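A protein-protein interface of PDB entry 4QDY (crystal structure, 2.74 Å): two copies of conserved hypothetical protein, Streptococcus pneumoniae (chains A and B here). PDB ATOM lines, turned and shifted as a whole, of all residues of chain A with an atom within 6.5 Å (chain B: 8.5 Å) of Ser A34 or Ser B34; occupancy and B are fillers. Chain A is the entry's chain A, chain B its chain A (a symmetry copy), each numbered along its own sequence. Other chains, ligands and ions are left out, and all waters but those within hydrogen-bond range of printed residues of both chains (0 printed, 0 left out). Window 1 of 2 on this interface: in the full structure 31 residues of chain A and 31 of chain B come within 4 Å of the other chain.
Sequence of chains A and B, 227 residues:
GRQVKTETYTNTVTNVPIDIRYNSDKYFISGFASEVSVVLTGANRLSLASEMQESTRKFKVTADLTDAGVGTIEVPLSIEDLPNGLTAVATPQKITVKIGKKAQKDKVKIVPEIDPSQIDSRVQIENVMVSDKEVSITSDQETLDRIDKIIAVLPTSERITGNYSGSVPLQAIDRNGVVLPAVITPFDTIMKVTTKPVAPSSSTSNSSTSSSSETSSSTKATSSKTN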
ATOM      1  N   VAL A  16       2.260 -10.389 -17.380  1.00  0.00           N
ATOM      2  CA  VAL A  16       3.599 -10.449 -17.978  1.00  0.00           C
ATOM      3  C   VAL A  16       4.456 -11.411 -17.129  1.00  0.00           C
ATOM      4  O   VAL A  16       4.763 -11.091 -15.978  1.00  0.00           O
ATOM      5  CB  VAL A  16       4.264  -9.051 -18.134  1.00  0.00           C
ATOM      6  CG1 VAL A  16       5.589  -9.156 -18.880  1.00  0.00           C
ATOM      7  CG2 VAL A  16       3.339  -8.079 -18.855  1.00  0.00           C
ATOM      8  N   PRO A  17       4.832 -12.599 -17.657  1.00  0.00           N
ATOM      9  CA  PRO A  17       5.633 -13.533 -16.845  1.00  0.00           C
ATOM     10  C   PRO A  17       7.097 -13.096 -16.739  1.00  0.00           C
ATOM     11  O   PRO A  17       7.634 -12.511 -17.680  1.00  0.00           O
ATOM     12  CB  PRO A  17       5.505 -14.860 -17.597  1.00  0.00           C
ATOM     13  CG  PRO A  17       5.235 -14.483 -19.006  1.00  0.00           C
ATOM     14  CD  PRO A  17       4.541 -13.150 -18.999  1.00  0.00           C
ATOM     15  N   ILE A  18       7.735 -13.394 -15.594  1.00  0.00           N
ATOM     16  CA  ILE A  18       9.131 -13.044 -15.302  1.00  0.00           C
ATOM     17  C   ILE A  18      10.050 -14.204 -15.703  1.00  0.00           C
ATOM     18  O   ILE A  18       9.801 -15.347 -15.309  1.00  0.00           O
ATOM     19  CB  ILE A  18       9.320 -12.680 -13.797  1.00  0.00           C
ATOM     20  CG1 ILE A  18       8.202 -11.747 -13.270  1.00  0.00           C
ATOM     21  CG2 ILE A  18      10.724 -12.105 -13.543  1.00  0.00           C
ATOM     22  CD1 ILE A  18       8.116 -11.645 -11.745  1.00  0.00           C
ATOM     23  N   ILE A  20      13.131 -15.722 -14.824  1.00  0.00           N
ATOM     24  CA  ILE A  20      14.094 -15.796 -13.730  1.00  0.00           C
ATOM     25  C   ILE A  20      15.209 -16.785 -14.074  1.00  0.00           C
ATOM     26  O   ILE A  20      14.941 -17.965 -14.301  1.00  0.00           O
ATOM     27  CB  ILE A  20      13.383 -16.193 -12.407  1.00  0.00           C
ATOM     28  CG1 ILE A  20      12.278 -15.170 -12.053  1.00  0.00           C
ATOM     29  CG2 ILE A  20      14.399 -16.335 -11.267  1.00  0.00           C
ATOM     30  CD1 ILE A  20      11.406 -15.514 -10.901  1.00  0.00           C
ATOM     31  N   TYR A  22      18.384 -18.863 -12.793  1.00  0.00           N
ATOM     32  CA  TYR A  22      18.925 -19.506 -11.592  1.00  0.00           C
ATOM     33  C   TYR A  22      19.154 -20.999 -11.847  1.00  0.00           C
ATOM     34  O   TYR A  22      18.502 -21.581 -12.720  1.00  0.00           O
ATOM     35  CB  TYR A  22      17.980 -19.305 -10.380  1.00  0.00           C
ATOM     36  CG  TYR A  22      16.727 -20.156 -10.397  1.00  0.00           C
ATOM     37  CD1 TYR A  22      15.668 -19.857 -11.250  1.00  0.00           C
ATOM     38  CD2 TYR A  22      16.567 -21.211  -9.503  1.00  0.00           C
ATOM     39  CE1 TYR A  22      14.514 -20.639 -11.270  1.00  0.00           C
ATOM     40  CE2 TYR A  22      15.405 -21.981  -9.493  1.00  0.00           C
ATOM     41  CZ  TYR A  22      14.381 -21.693 -10.380  1.00  0.00           C
ATOM     42  OH  TYR A  22      13.234 -22.451 -10.365  1.00  0.00           O
ATOM     43  N   ILE A  29      13.277 -22.012  -5.430  1.00  0.00           N
ATOM     44  CA  ILE A  29      12.869 -20.632  -5.149  1.00  0.00           C
ATOM     45  C   ILE A  29      11.333 -20.536  -4.985  1.00  0.00           C
ATOM     46  O   ILE A  29      10.587 -21.318  -5.582  1.00  0.00           O
ATOM     47  CB  ILE A  29      13.372 -19.639  -6.240  1.00  0.00           C
ATOM     48  CG1 ILE A  29      12.766 -19.923  -7.641  1.00  0.00           C
ATOM     49  CG2 ILE A  29      14.915 -19.588  -6.268  1.00  0.00           C
ATOM     50  CD1 ILE A  29      12.975 -18.816  -8.677  1.00  0.00           C
ATOM     51  N   PHE A  32       7.267 -15.106  -4.378  1.00  0.00           N
ATOM     52  CA  PHE A  32       7.073 -13.997  -5.317  1.00  0.00           C
ATOM     53  C   PHE A  32       5.888 -14.261  -6.246  1.00  0.00           C
ATOM     54  O   PHE A  32       5.515 -15.420  -6.451  1.00  0.00           O
ATOM     55  CB  PHE A  32       8.353 -13.769  -6.152  1.00  0.00           C
ATOM     56  CG  PHE A  32       8.860 -15.012  -6.848  1.00  0.00           C
ATOM     57  CD1 PHE A  32       8.379 -15.374  -8.100  1.00  0.00           C
ATOM     58  CD2 PHE A  32       9.804 -15.832  -6.240  1.00  0.00           C
ATOM     59  CE1 PHE A  32       8.806 -16.549  -8.715  1.00  0.00           C
ATOM     60  CE2 PHE A  32      10.240 -17.001  -6.863  1.00  0.00           C
ATOM     61  CZ  PHE A  32       9.741 -17.349  -8.097  1.00  0.00           C
ATOM     62  N   ALA A  33       5.318 -13.192  -6.832  1.00  0.00           N
ATOM     63  CA  ALA A  33       4.221 -13.307  -7.792  1.00  0.00           C
ATOM     64  C   ALA A  33       4.786 -13.651  -9.164  1.00  0.00           C
ATOM     65  O   ALA A  33       5.655 -12.931  -9.669  1.00  0.00           O
ATOM     66  CB  ALA A  33       3.412 -12.019  -7.837  1.00  0.00           C
ATOM     67  N   SER A  34       4.325 -14.781  -9.737  1.00  0.00           N
ATOM     68  CA  SER A  34       4.749 -15.342 -11.030  1.00  0.00           C
ATOM     69  C   SER A  34       4.701 -14.325 -12.175  1.00  0.00           C
ATOM     70  O   SER A  34       5.573 -14.356 -13.045  1.00  0.00           O
ATOM     71  CB  SER A  34       3.858 -16.523 -11.405  1.00  0.00           C
ATOM     72  OG  SER A  34       2.502 -16.135 -11.559  1.00  0.00           O
ATOM     73  N   GLU A  35       3.670 -13.454 -12.190  1.00  0.00           N
ATOM     74  CA  GLU A  35       3.478 -12.468 -13.247  1.00  0.00           C
ATOM     75  C   GLU A  35       3.416 -11.042 -12.697  1.00  0.00           C
ATOM     76  O   GLU A  35       3.045 -10.824 -11.542  1.00  0.00           O
ATOM     77  CB  GLU A  35       2.196 -12.767 -14.041  1.00  0.00           C
ATOM     78  CG  GLU A  35       2.287 -14.032 -14.882  1.00  0.00           C
ATOM     79  CD  GLU A  35       1.071 -14.392 -15.713  1.00  0.00           C
ATOM     80  OE1 GLU A  35      -0.063 -14.036 -15.317  1.00  0.00           O
ATOM     81  OE2 GLU A  35       1.250 -15.096 -16.732  1.00  0.00           O
ATOM     82  N   VAL A  36       3.794 -10.075 -13.551  1.00  0.00           N
ATOM     83  CA  VAL A  36       3.817  -8.638 -13.257  1.00  0.00           C
ATOM     84  C   VAL A  36       3.027  -7.868 -14.328  1.00  0.00           C
ATOM     85  O   VAL A  36       2.564  -8.452 -15.310  1.00  0.00           O
ATOM     86  CB  VAL A  36       5.271  -8.080 -13.146  1.00  0.00           C
ATOM     87  CG1 VAL A  36       6.002  -8.642 -11.935  1.00  0.00           C
ATOM     88  CG2 VAL A  36       6.074  -8.299 -14.430  1.00  0.00           C
ATOM     89  N   ASN B  15      13.897 -23.126 -16.543  1.00  0.00           N
ATOM     90  CA  ASN B  15      13.493 -21.746 -16.240  1.00  0.00           C
ATOM     91  C   ASN B  15      12.566 -21.191 -17.349  1.00  0.00           C
ATOM     92  O   ASN B  15      12.794 -20.087 -17.859  1.00  0.00           O
ATOM     93  CB  ASN B  15      14.732 -20.834 -16.056  1.00  0.00           C
ATOM     94  CG  ASN B  15      15.746 -21.304 -15.033  1.00  0.00           C
ATOM     95  OD1 ASN B  15      15.558 -22.297 -14.318  1.00  0.00           O
ATOM     96  ND2 ASN B  15      16.861 -20.596 -14.952  1.00  0.00           N
ATOM     97  N   VAL B  16      11.516 -21.958 -17.711  1.00  0.00           N
ATOM     98  CA  VAL B  16      10.568 -21.539 -18.750  1.00  0.00           C
ATOM     99  C   VAL B  16       9.342 -20.916 -18.050  1.00  0.00           C
ATOM    100  O   VAL B  16       8.600 -21.637 -17.378  1.00  0.00           O
ATOM    101  CB  VAL B  16      10.171 -22.690 -19.719  1.00  0.00           C
ATOM    102  CG1 VAL B  16       9.295 -22.172 -20.853  1.00  0.00           C
ATOM    103  CG2 VAL B  16      11.404 -23.379 -20.289  1.00  0.00           C
ATOM    104  N   PRO B  17       9.120 -19.587 -18.168  1.00  0.00           N
ATOM    105  CA  PRO B  17       7.962 -18.981 -17.485  1.00  0.00           C
ATOM    106  C   PRO B  17       6.645 -19.283 -18.205  1.00  0.00           C
ATOM    107  O   PRO B  17       6.625 -19.392 -19.431  1.00  0.00           O
ATOM    108  CB  PRO B  17       8.276 -17.483 -17.511  1.00  0.00           C
ATOM    109  CG  PRO B  17       9.162 -17.294 -18.686  1.00  0.00           C
ATOM    110  CD  PRO B  17       9.908 -18.579 -18.910  1.00  0.00           C
ATOM    111  N   ILE B  18       5.549 -19.405 -17.435  1.00  0.00           N
ATOM    112  CA  ILE B  18       4.205 -19.709 -17.940  1.00  0.00           C
ATOM    113  C   ILE B  18       3.444 -18.404 -18.200  1.00  0.00           C
ATOM    114  O   ILE B  18       3.388 -17.540 -17.320  1.00  0.00           O
ATOM    115  CB  ILE B  18       3.420 -20.621 -16.947  1.00  0.00           C
ATOM    116  CG1 ILE B  18       4.284 -21.788 -16.408  1.00  0.00           C
ATOM    117  CG2 ILE B  18       2.105 -21.113 -17.575  1.00  0.00           C
ATOM    118  CD1 ILE B  18       3.712 -22.494 -15.176  1.00  0.00           C
ATOM    119  N   ASP B  19       2.838 -18.274 -19.395  1.00  0.00           N
ATOM    120  CA  ASP B  19       2.051 -17.095 -19.737  1.00  0.00           C
ATOM    121  C   ASP B  19       0.586 -17.418 -19.432  1.00  0.00           C
ATOM    122  O   ASP B  19      -0.120 -18.006 -20.251  1.00  0.00           O
ATOM    123  CB  ASP B  19       2.288 -16.670 -21.202  1.00  0.00           C
ATOM    124  CG  ASP B  19       1.817 -15.264 -21.547  1.00  0.00           C
ATOM    125  OD1 ASP B  19       0.655 -14.923 -21.218  1.00  0.00           O
ATOM    126  OD2 ASP B  19       2.584 -14.527 -22.203  1.00  0.00           O
ATOM    127  N   ILE B  20       0.156 -17.075 -18.216  1.00  0.00           N
ATOM    128  CA  ILE B  20      -1.187 -17.350 -17.715  1.00  0.00           C
ATOM    129  C   ILE B  20      -2.132 -16.206 -18.083  1.00  0.00           C
ATOM    130  O   ILE B  20      -1.905 -15.064 -17.683  1.00  0.00           O
ATOM    131  CB  ILE B  20      -1.158 -17.581 -16.179  1.00  0.00           C
ATOM    132  CG1 ILE B  20      -0.222 -18.760 -15.822  1.00  0.00           C
ATOM    133  CG2 ILE B  20      -2.575 -17.808 -15.639  1.00  0.00           C
ATOM    134  CD1 ILE B  20       0.030 -18.986 -14.376  1.00  0.00           C
ATOM    135  N   TYR B  22      -5.730 -14.517 -17.590  1.00  0.00           N
ATOM    136  CA  TYR B  22      -6.795 -14.355 -16.596  1.00  0.00           C
ATOM    137  C   TYR B  22      -7.032 -12.870 -16.308  1.00  0.00           C
ATOM    138  O   TYR B  22      -6.125 -12.054 -16.503  1.00  0.00           O
ATOM    139  CB  TYR B  22      -6.451 -15.110 -15.286  1.00  0.00           C
ATOM    140  CG  TYR B  22      -5.401 -14.445 -14.420  1.00  0.00           C
ATOM    141  CD1 TYR B  22      -4.054 -14.479 -14.773  1.00  0.00           C
ATOM    142  CD2 TYR B  22      -5.743 -13.853 -13.208  1.00  0.00           C
ATOM    143  CE1 TYR B  22      -3.084 -13.867 -13.981  1.00  0.00           C
ATOM    144  CE2 TYR B  22      -4.778 -13.264 -12.394  1.00  0.00           C
ATOM    145  CZ  TYR B  22      -3.449 -13.271 -12.784  1.00  0.00           C
ATOM    146  OH  TYR B  22      -2.498 -12.694 -11.976  1.00  0.00           O
ATOM    147  N   ILE B  29      -4.626 -15.051  -8.172  1.00  0.00           N
ATOM    148  CA  ILE B  29      -4.250 -16.461  -8.317  1.00  0.00           C
ATOM    149  C   ILE B  29      -2.933 -16.759  -7.559  1.00  0.00           C
ATOM    150  O   ILE B  29      -2.081 -15.879  -7.409  1.00  0.00           O
ATOM    151  CB  ILE B  29      -4.136 -16.886  -9.812  1.00  0.00           C
ATOM    152  CG1 ILE B  29      -3.015 -16.128 -10.572  1.00  0.00           C
ATOM    153  CG2 ILE B  29      -5.503 -16.776 -10.520  1.00  0.00           C
ATOM    154  CD1 ILE B  29      -2.650 -16.707 -11.941  1.00  0.00           C
ATOM    155  N   SER B  30      -2.796 -18.019  -7.080  1.00  0.00           N
ATOM    156  CA  SER B  30      -1.644 -18.547  -6.333  1.00  0.00           C
ATOM    157  C   SER B  30      -1.671 -20.087  -6.271  1.00  0.00           C
ATOM    158  O   SER B  30      -2.651 -20.706  -6.693  1.00  0.00           O
ATOM    159  CB  SER B  30      -1.622 -17.978  -4.913  1.00  0.00           C
ATOM    160  OG  SER B  30      -2.765 -18.375  -4.171  1.00  0.00           O
ATOM    161  N   GLY B  31      -0.600 -20.677  -5.731  1.00  0.00           N
ATOM    162  CA  GLY B  31      -0.489 -22.118  -5.516  1.00  0.00           C
ATOM    163  C   GLY B  31       0.135 -22.958  -6.613  1.00  0.00           C
ATOM    164  O   GLY B  31      -0.104 -24.168  -6.663  1.00  0.00           O
ATOM    165  N   PHE B  32       0.966 -22.342  -7.469  1.00  0.00           N
ATOM    166  CA  PHE B  32       1.650 -23.000  -8.587  1.00  0.00           C
ATOM    167  C   PHE B  32       3.090 -22.502  -8.722  1.00  0.00           C
ATOM    168  O   PHE B  32       3.403 -21.398  -8.267  1.00  0.00           O
ATOM    169  CB  PHE B  32       0.884 -22.755  -9.905  1.00  0.00           C
ATOM    170  CG  PHE B  32       0.612 -21.296 -10.194  1.00  0.00           C
ATOM    171  CD1 PHE B  32       1.550 -20.513 -10.857  1.00  0.00           C
ATOM    172  CD2 PHE B  32      -0.575 -20.700  -9.783  1.00  0.00           C
ATOM    173  CE1 PHE B  32       1.320 -19.156 -11.072  1.00  0.00           C
ATOM    174  CE2 PHE B  32      -0.808 -19.343 -10.012  1.00  0.00           C
ATOM    175  CZ  PHE B  32       0.140 -18.583 -10.658  1.00  0.00           C
ATOM    176  N   ALA B  33       3.955 -23.299  -9.376  1.00  0.00           N
ATOM    177  CA  ALA B  33       5.343 -22.917  -9.634  1.00  0.00           C
ATOM    178  C   ALA B  33       5.395 -22.004 -10.851  1.00  0.00           C
ATOM    179  O   ALA B  33       4.902 -22.379 -11.922  1.00  0.00           O
ATOM    180  CB  ALA B  33       6.210 -24.152  -9.832  1.00  0.00           C
ATOM    181  N   SER B  34       5.949 -20.789 -10.668  1.00  0.00           N
ATOM    182  CA  SER B  34       6.074 -19.723 -11.675  1.00  0.00           C
ATOM    183  C   SER B  34       6.708 -20.201 -12.986  1.00  0.00           C
ATOM    184  O   SER B  34       6.298 -19.744 -14.055  1.00  0.00           O
ATOM    185  CB  SER B  34       6.923 -18.581 -11.125  1.00  0.00           C
ATOM    186  OG  SER B  34       8.242 -19.002 -10.819  1.00  0.00           O
ATOM    187  N   GLU B  35       7.721 -21.088 -12.899  1.00  0.00           N
ATOM    188  CA  GLU B  35       8.443 -21.586 -14.064  1.00  0.00           C
ATOM    189  C   GLU B  35       8.396 -23.112 -14.158  1.00  0.00           C
ATOM    190  O   GLU B  35       8.252 -23.805 -13.149  1.00  0.00           O
ATOM    191  CB  GLU B  35       9.908 -21.119 -14.035  1.00  0.00           C
ATOM    192  CG  GLU B  35      10.069 -19.622 -14.253  1.00  0.00           C
ATOM    193  CD  GLU B  35      11.485 -19.078 -14.258  1.00  0.00           C
ATOM    194  OE1 GLU B  35      12.364 -19.668 -13.589  1.00  0.00           O
ATOM    195  OE2 GLU B  35      11.697 -18.014 -14.881  1.00  0.00           O
ATOM    196  N   VAL B  36       8.517 -23.620 -15.397  1.00  0.00           N
ATOM    197  CA  VAL B  36       8.507 -25.046 -15.740  1.00  0.00           C
ATOM    198  C   VAL B  36       9.750 -25.398 -16.572  1.00  0.00           C
ATOM    199  O   VAL B  36      10.534 -24.520 -16.935  1.00  0.00           O
ATOM    200  CB  VAL B  36       7.207 -25.462 -16.499  1.00  0.00           C
ATOM    201  CG1 VAL B  36       5.974 -25.360 -15.610  1.00  0.00           C
ATOM    202  CG2 VAL B  36       7.020 -24.676 -17.798  1.00  0.00           C
ATOM    203  N   SER B  37       9.911 -26.692 -16.874  1.00  0.00           N
ATOM    204  CA  SER B  37      10.953 -27.214 -17.752  1.00  0.00           C
ATOM    205  C   SER B  37      10.289 -27.780 -18.999  1.00  0.00           C
ATOM    206  O   SER B  37       9.184 -28.313 -18.908  1.00  0.00           O
ATOM    207  CB  SER B  37      11.820 -28.253 -17.048  1.00  0.00           C
ATOM    208  OG  SER B  37      12.605 -27.646 -16.035  1.00  0.00           O
ATOM    209  N   VAL B  61       5.066 -21.250 -23.248  1.00  0.00           N
ATOM    210  CA  VAL B  61       4.162 -22.144 -22.527  1.00  0.00           C
ATOM    211  C   VAL B  61       3.050 -21.250 -21.943  1.00  0.00           C
ATOM    212  O   VAL B  61       3.333 -20.250 -21.278  1.00  0.00           O
ATOM    213  CB  VAL B  61       4.848 -23.065 -21.477  1.00  0.00           C
ATOM    214  CG1 VAL B  61       5.631 -22.282 -20.432  1.00  0.00           C
ATOM    215  CG2 VAL B  61       3.846 -24.006 -20.816  1.00  0.00           C
ATOM    216  N   LEU B  77      -1.246 -27.084 -19.594  1.00  0.00           N
ATOM    217  CA  LEU B  77      -0.361 -26.100 -20.213  1.00  0.00           C
ATOM    218  C   LEU B  77      -0.271 -26.339 -21.723  1.00  0.00           C
ATOM    219  O   LEU B  77      -0.286 -27.493 -22.161  1.00  0.00           O
ATOM    220  CB  LEU B  77       1.046 -26.134 -19.584  1.00  0.00           C
ATOM    221  CG  LEU B  77       1.182 -25.877 -18.076  1.00  0.00           C
ATOM    222  CD1 LEU B  77       2.634 -25.930 -17.658  1.00  0.00           C
ATOM    223  CD2 LEU B  77       0.607 -24.529 -17.674  1.00  0.00           C
ATOM    224  N   ILE B  95      -0.778 -27.423 -14.207  1.00  0.00           N
ATOM    225  CA  ILE B  95      -0.470 -26.637 -13.004  1.00  0.00           C
ATOM    226  C   ILE B  95      -1.752 -26.490 -12.170  1.00  0.00           C
ATOM    227  O   ILE B  95      -2.845 -26.435 -12.732  1.00  0.00           O
ATOM    228  CB  ILE B  95       0.178 -25.247 -13.307  1.00  0.00           C
ATOM    229  CG1 ILE B  95      -0.765 -24.300 -14.109  1.00  0.00           C
ATOM    230  CG2 ILE B  95       1.554 -25.418 -13.979  1.00  0.00           C
ATOM    231  CD1 ILE B  95      -0.326 -22.822 -14.216  1.00  0.00           C
ATOM    232  N   VAL B  97      -3.993 -24.177  -9.808  1.00  0.00           N
ATOM    233  CA  VAL B  97      -4.201 -22.754  -9.543  1.00  0.00           C
ATOM    234  C   VAL B  97      -5.389 -22.556  -8.585  1.00  0.00           C
ATOM    235  O   VAL B  97      -6.456 -23.139  -8.794  1.00  0.00           O
ATOM    236  CB  VAL B  97      -4.425 -21.967 -10.869  1.00  0.00           C
ATOM    237  CG1 VAL B  97      -4.557 -20.472 -10.612  1.00  0.00           C
ATOM    238  CG2 VAL B  97      -3.303 -22.223 -11.873  1.00  0.00           C
ATOM    239  N   VAL B 183       0.288  -9.759  -2.349  1.00  0.00           N
ATOM    240  CA  VAL B 183       1.056  -8.692  -3.001  1.00  0.00           C
ATOM    241  C   VAL B 183       0.961  -7.443  -2.117  1.00  0.00           C
ATOM    242  O   VAL B 183      -0.137  -6.937  -1.885  1.00  0.00           O
ATOM    243  CB  VAL B 183       0.565  -8.436  -4.454  1.00  0.00           C
ATOM    244  CG1 VAL B 183       1.375  -7.331  -5.125  1.00  0.00           C
ATOM    245  CG2 VAL B 183       0.617  -9.711  -5.287  1.00  0.00           C
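The backbone carbonyl oxygen of Ile A20 sits at hydrogen-bond distance from the side-chain amide nitrogen of Asn B15.
OE2 of Glu B35 sits at hydrogen-bond distance from N of Ile A20 (2.7 Å).
The backbone carbonyl oxygen (O) of Tyr A22 lies within hydrogen-bond range of the side-chain amide nitrogen (ND2) of Asn B15 (2.9 Å).
The side-chain carboxylate of Glu A35 sits at hydrogen-bond distance from the backbone NH of Ile B20 (2.7 Å).
The backbone carbonyl oxygen (O) of Ile A18 lies close to the side-chain carboxylate (OE2) of Glu B35.
The side-chain carboxylate (OE2) of Glu A35 sits close to the backbone carbonyl oxygen (O) of Ile B18.
The backbone NH (N) of Ile A18 sits at hydrogen-bond distance from the backbone carbonyl oxygen (O) of Ser A34 (3.5 Å).
The backbone NH (N) of Ile B18 lies within hydrogen-bond range of the backbone carbonyl oxygen (O) of Ser B34, 3.5 Å away.
The backbone carbonyl oxygen (O) of Val B61 sits at hydrogen-bond distance from the backbone NH (N) of Asp B19 (2.8 Å).
Pro B17 touches Pro A17.
CB of Pro A17 touches O of Ile B18, at 3.4 Å.
Pro A17 touches Asp B19 (CD to OD2, 3.999 Å).
O of Ile A18 touches CB of Pro B17 (3.4 Å).
Tyr A22 touches Glu B35.
OG of Ser B34 touches CE1 of Phe A32 (3.3 Å).
OG of Ser A34 touches CE1 of Phe B32, at 3.3 Å.
Ser A34 touches Ser B34.
Glu A35 touches Asp B19 (OE2 to C, 3.6 Å).
Glu A35 touches Tyr B22.
Pro A17 touches Ile B18, and with the chains exchanged Ile A18 touches Pro B17.
Ile A20 touches Glu B35, and with the chains exchanged Glu A35 touches Ile B20.
Phe A32 touches Ser B34, and with the chains exchanged Ser A34 touches Phe B32.
Ser A34 touches its own counterpart, Ser B34.
Positions printed for both chains: 16, 17, 18, 20, 22, 29, 32, 33, 34, 35 and 36.
Of the 16 pairs that touch across the chains among the printed residues, 12 have their exchanged pair printed and touching as well.
Ser B34 touches just these residues of chain A: Phe A32 and Ser A34.
Printed residues of chain B within 4 Å of Ile A18: Pro B17 (3.4 Å) and Glu B35 (3.3 Å).
Of the printed residues of chain A, Glu B35 touches Ile A18 (3.3 Å), Ile A20 (2.7 Å) and Tyr A22 (3.3 Å).
Printed residues of chain B within 4 Å of Phe A32: Ser B34 (3.3 Å).
The nearest residue of chain B that does not touch Ser A34 is Ile B20 (4.7 Å).
The nearest residue of chain A that does not touch Ser B34 is Ile A20 (4.7 Å).
Of the 21 printed residues of chain B, 9 touch a printed residue of chain A.
Printed residues of chain B that touch a printed residue of chain A: Asn B15, Pro B17, Ile B18, Asp B19, Ile B20, Tyr B22, Phe B32, Ser B34 and Glu B35.
Hydrophobic or aromatic side chains of chain B that line the printed part of chain A: Pro B17, Ile B20, Tyr B22 and Phe B32.
Of the 11 printed residues of chain A, 7 touch a printed residue of chain B.
Hydrophobic or aromatic side chains of chain A that line the printed part of chain B: Pro A17, Ile A20, Tyr A22 and Phe A32.
Among the printed residues, no Asp or Glu carboxylate lies within 4 Å of a Lys or Arg side-chain nitrogen of the other chain.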
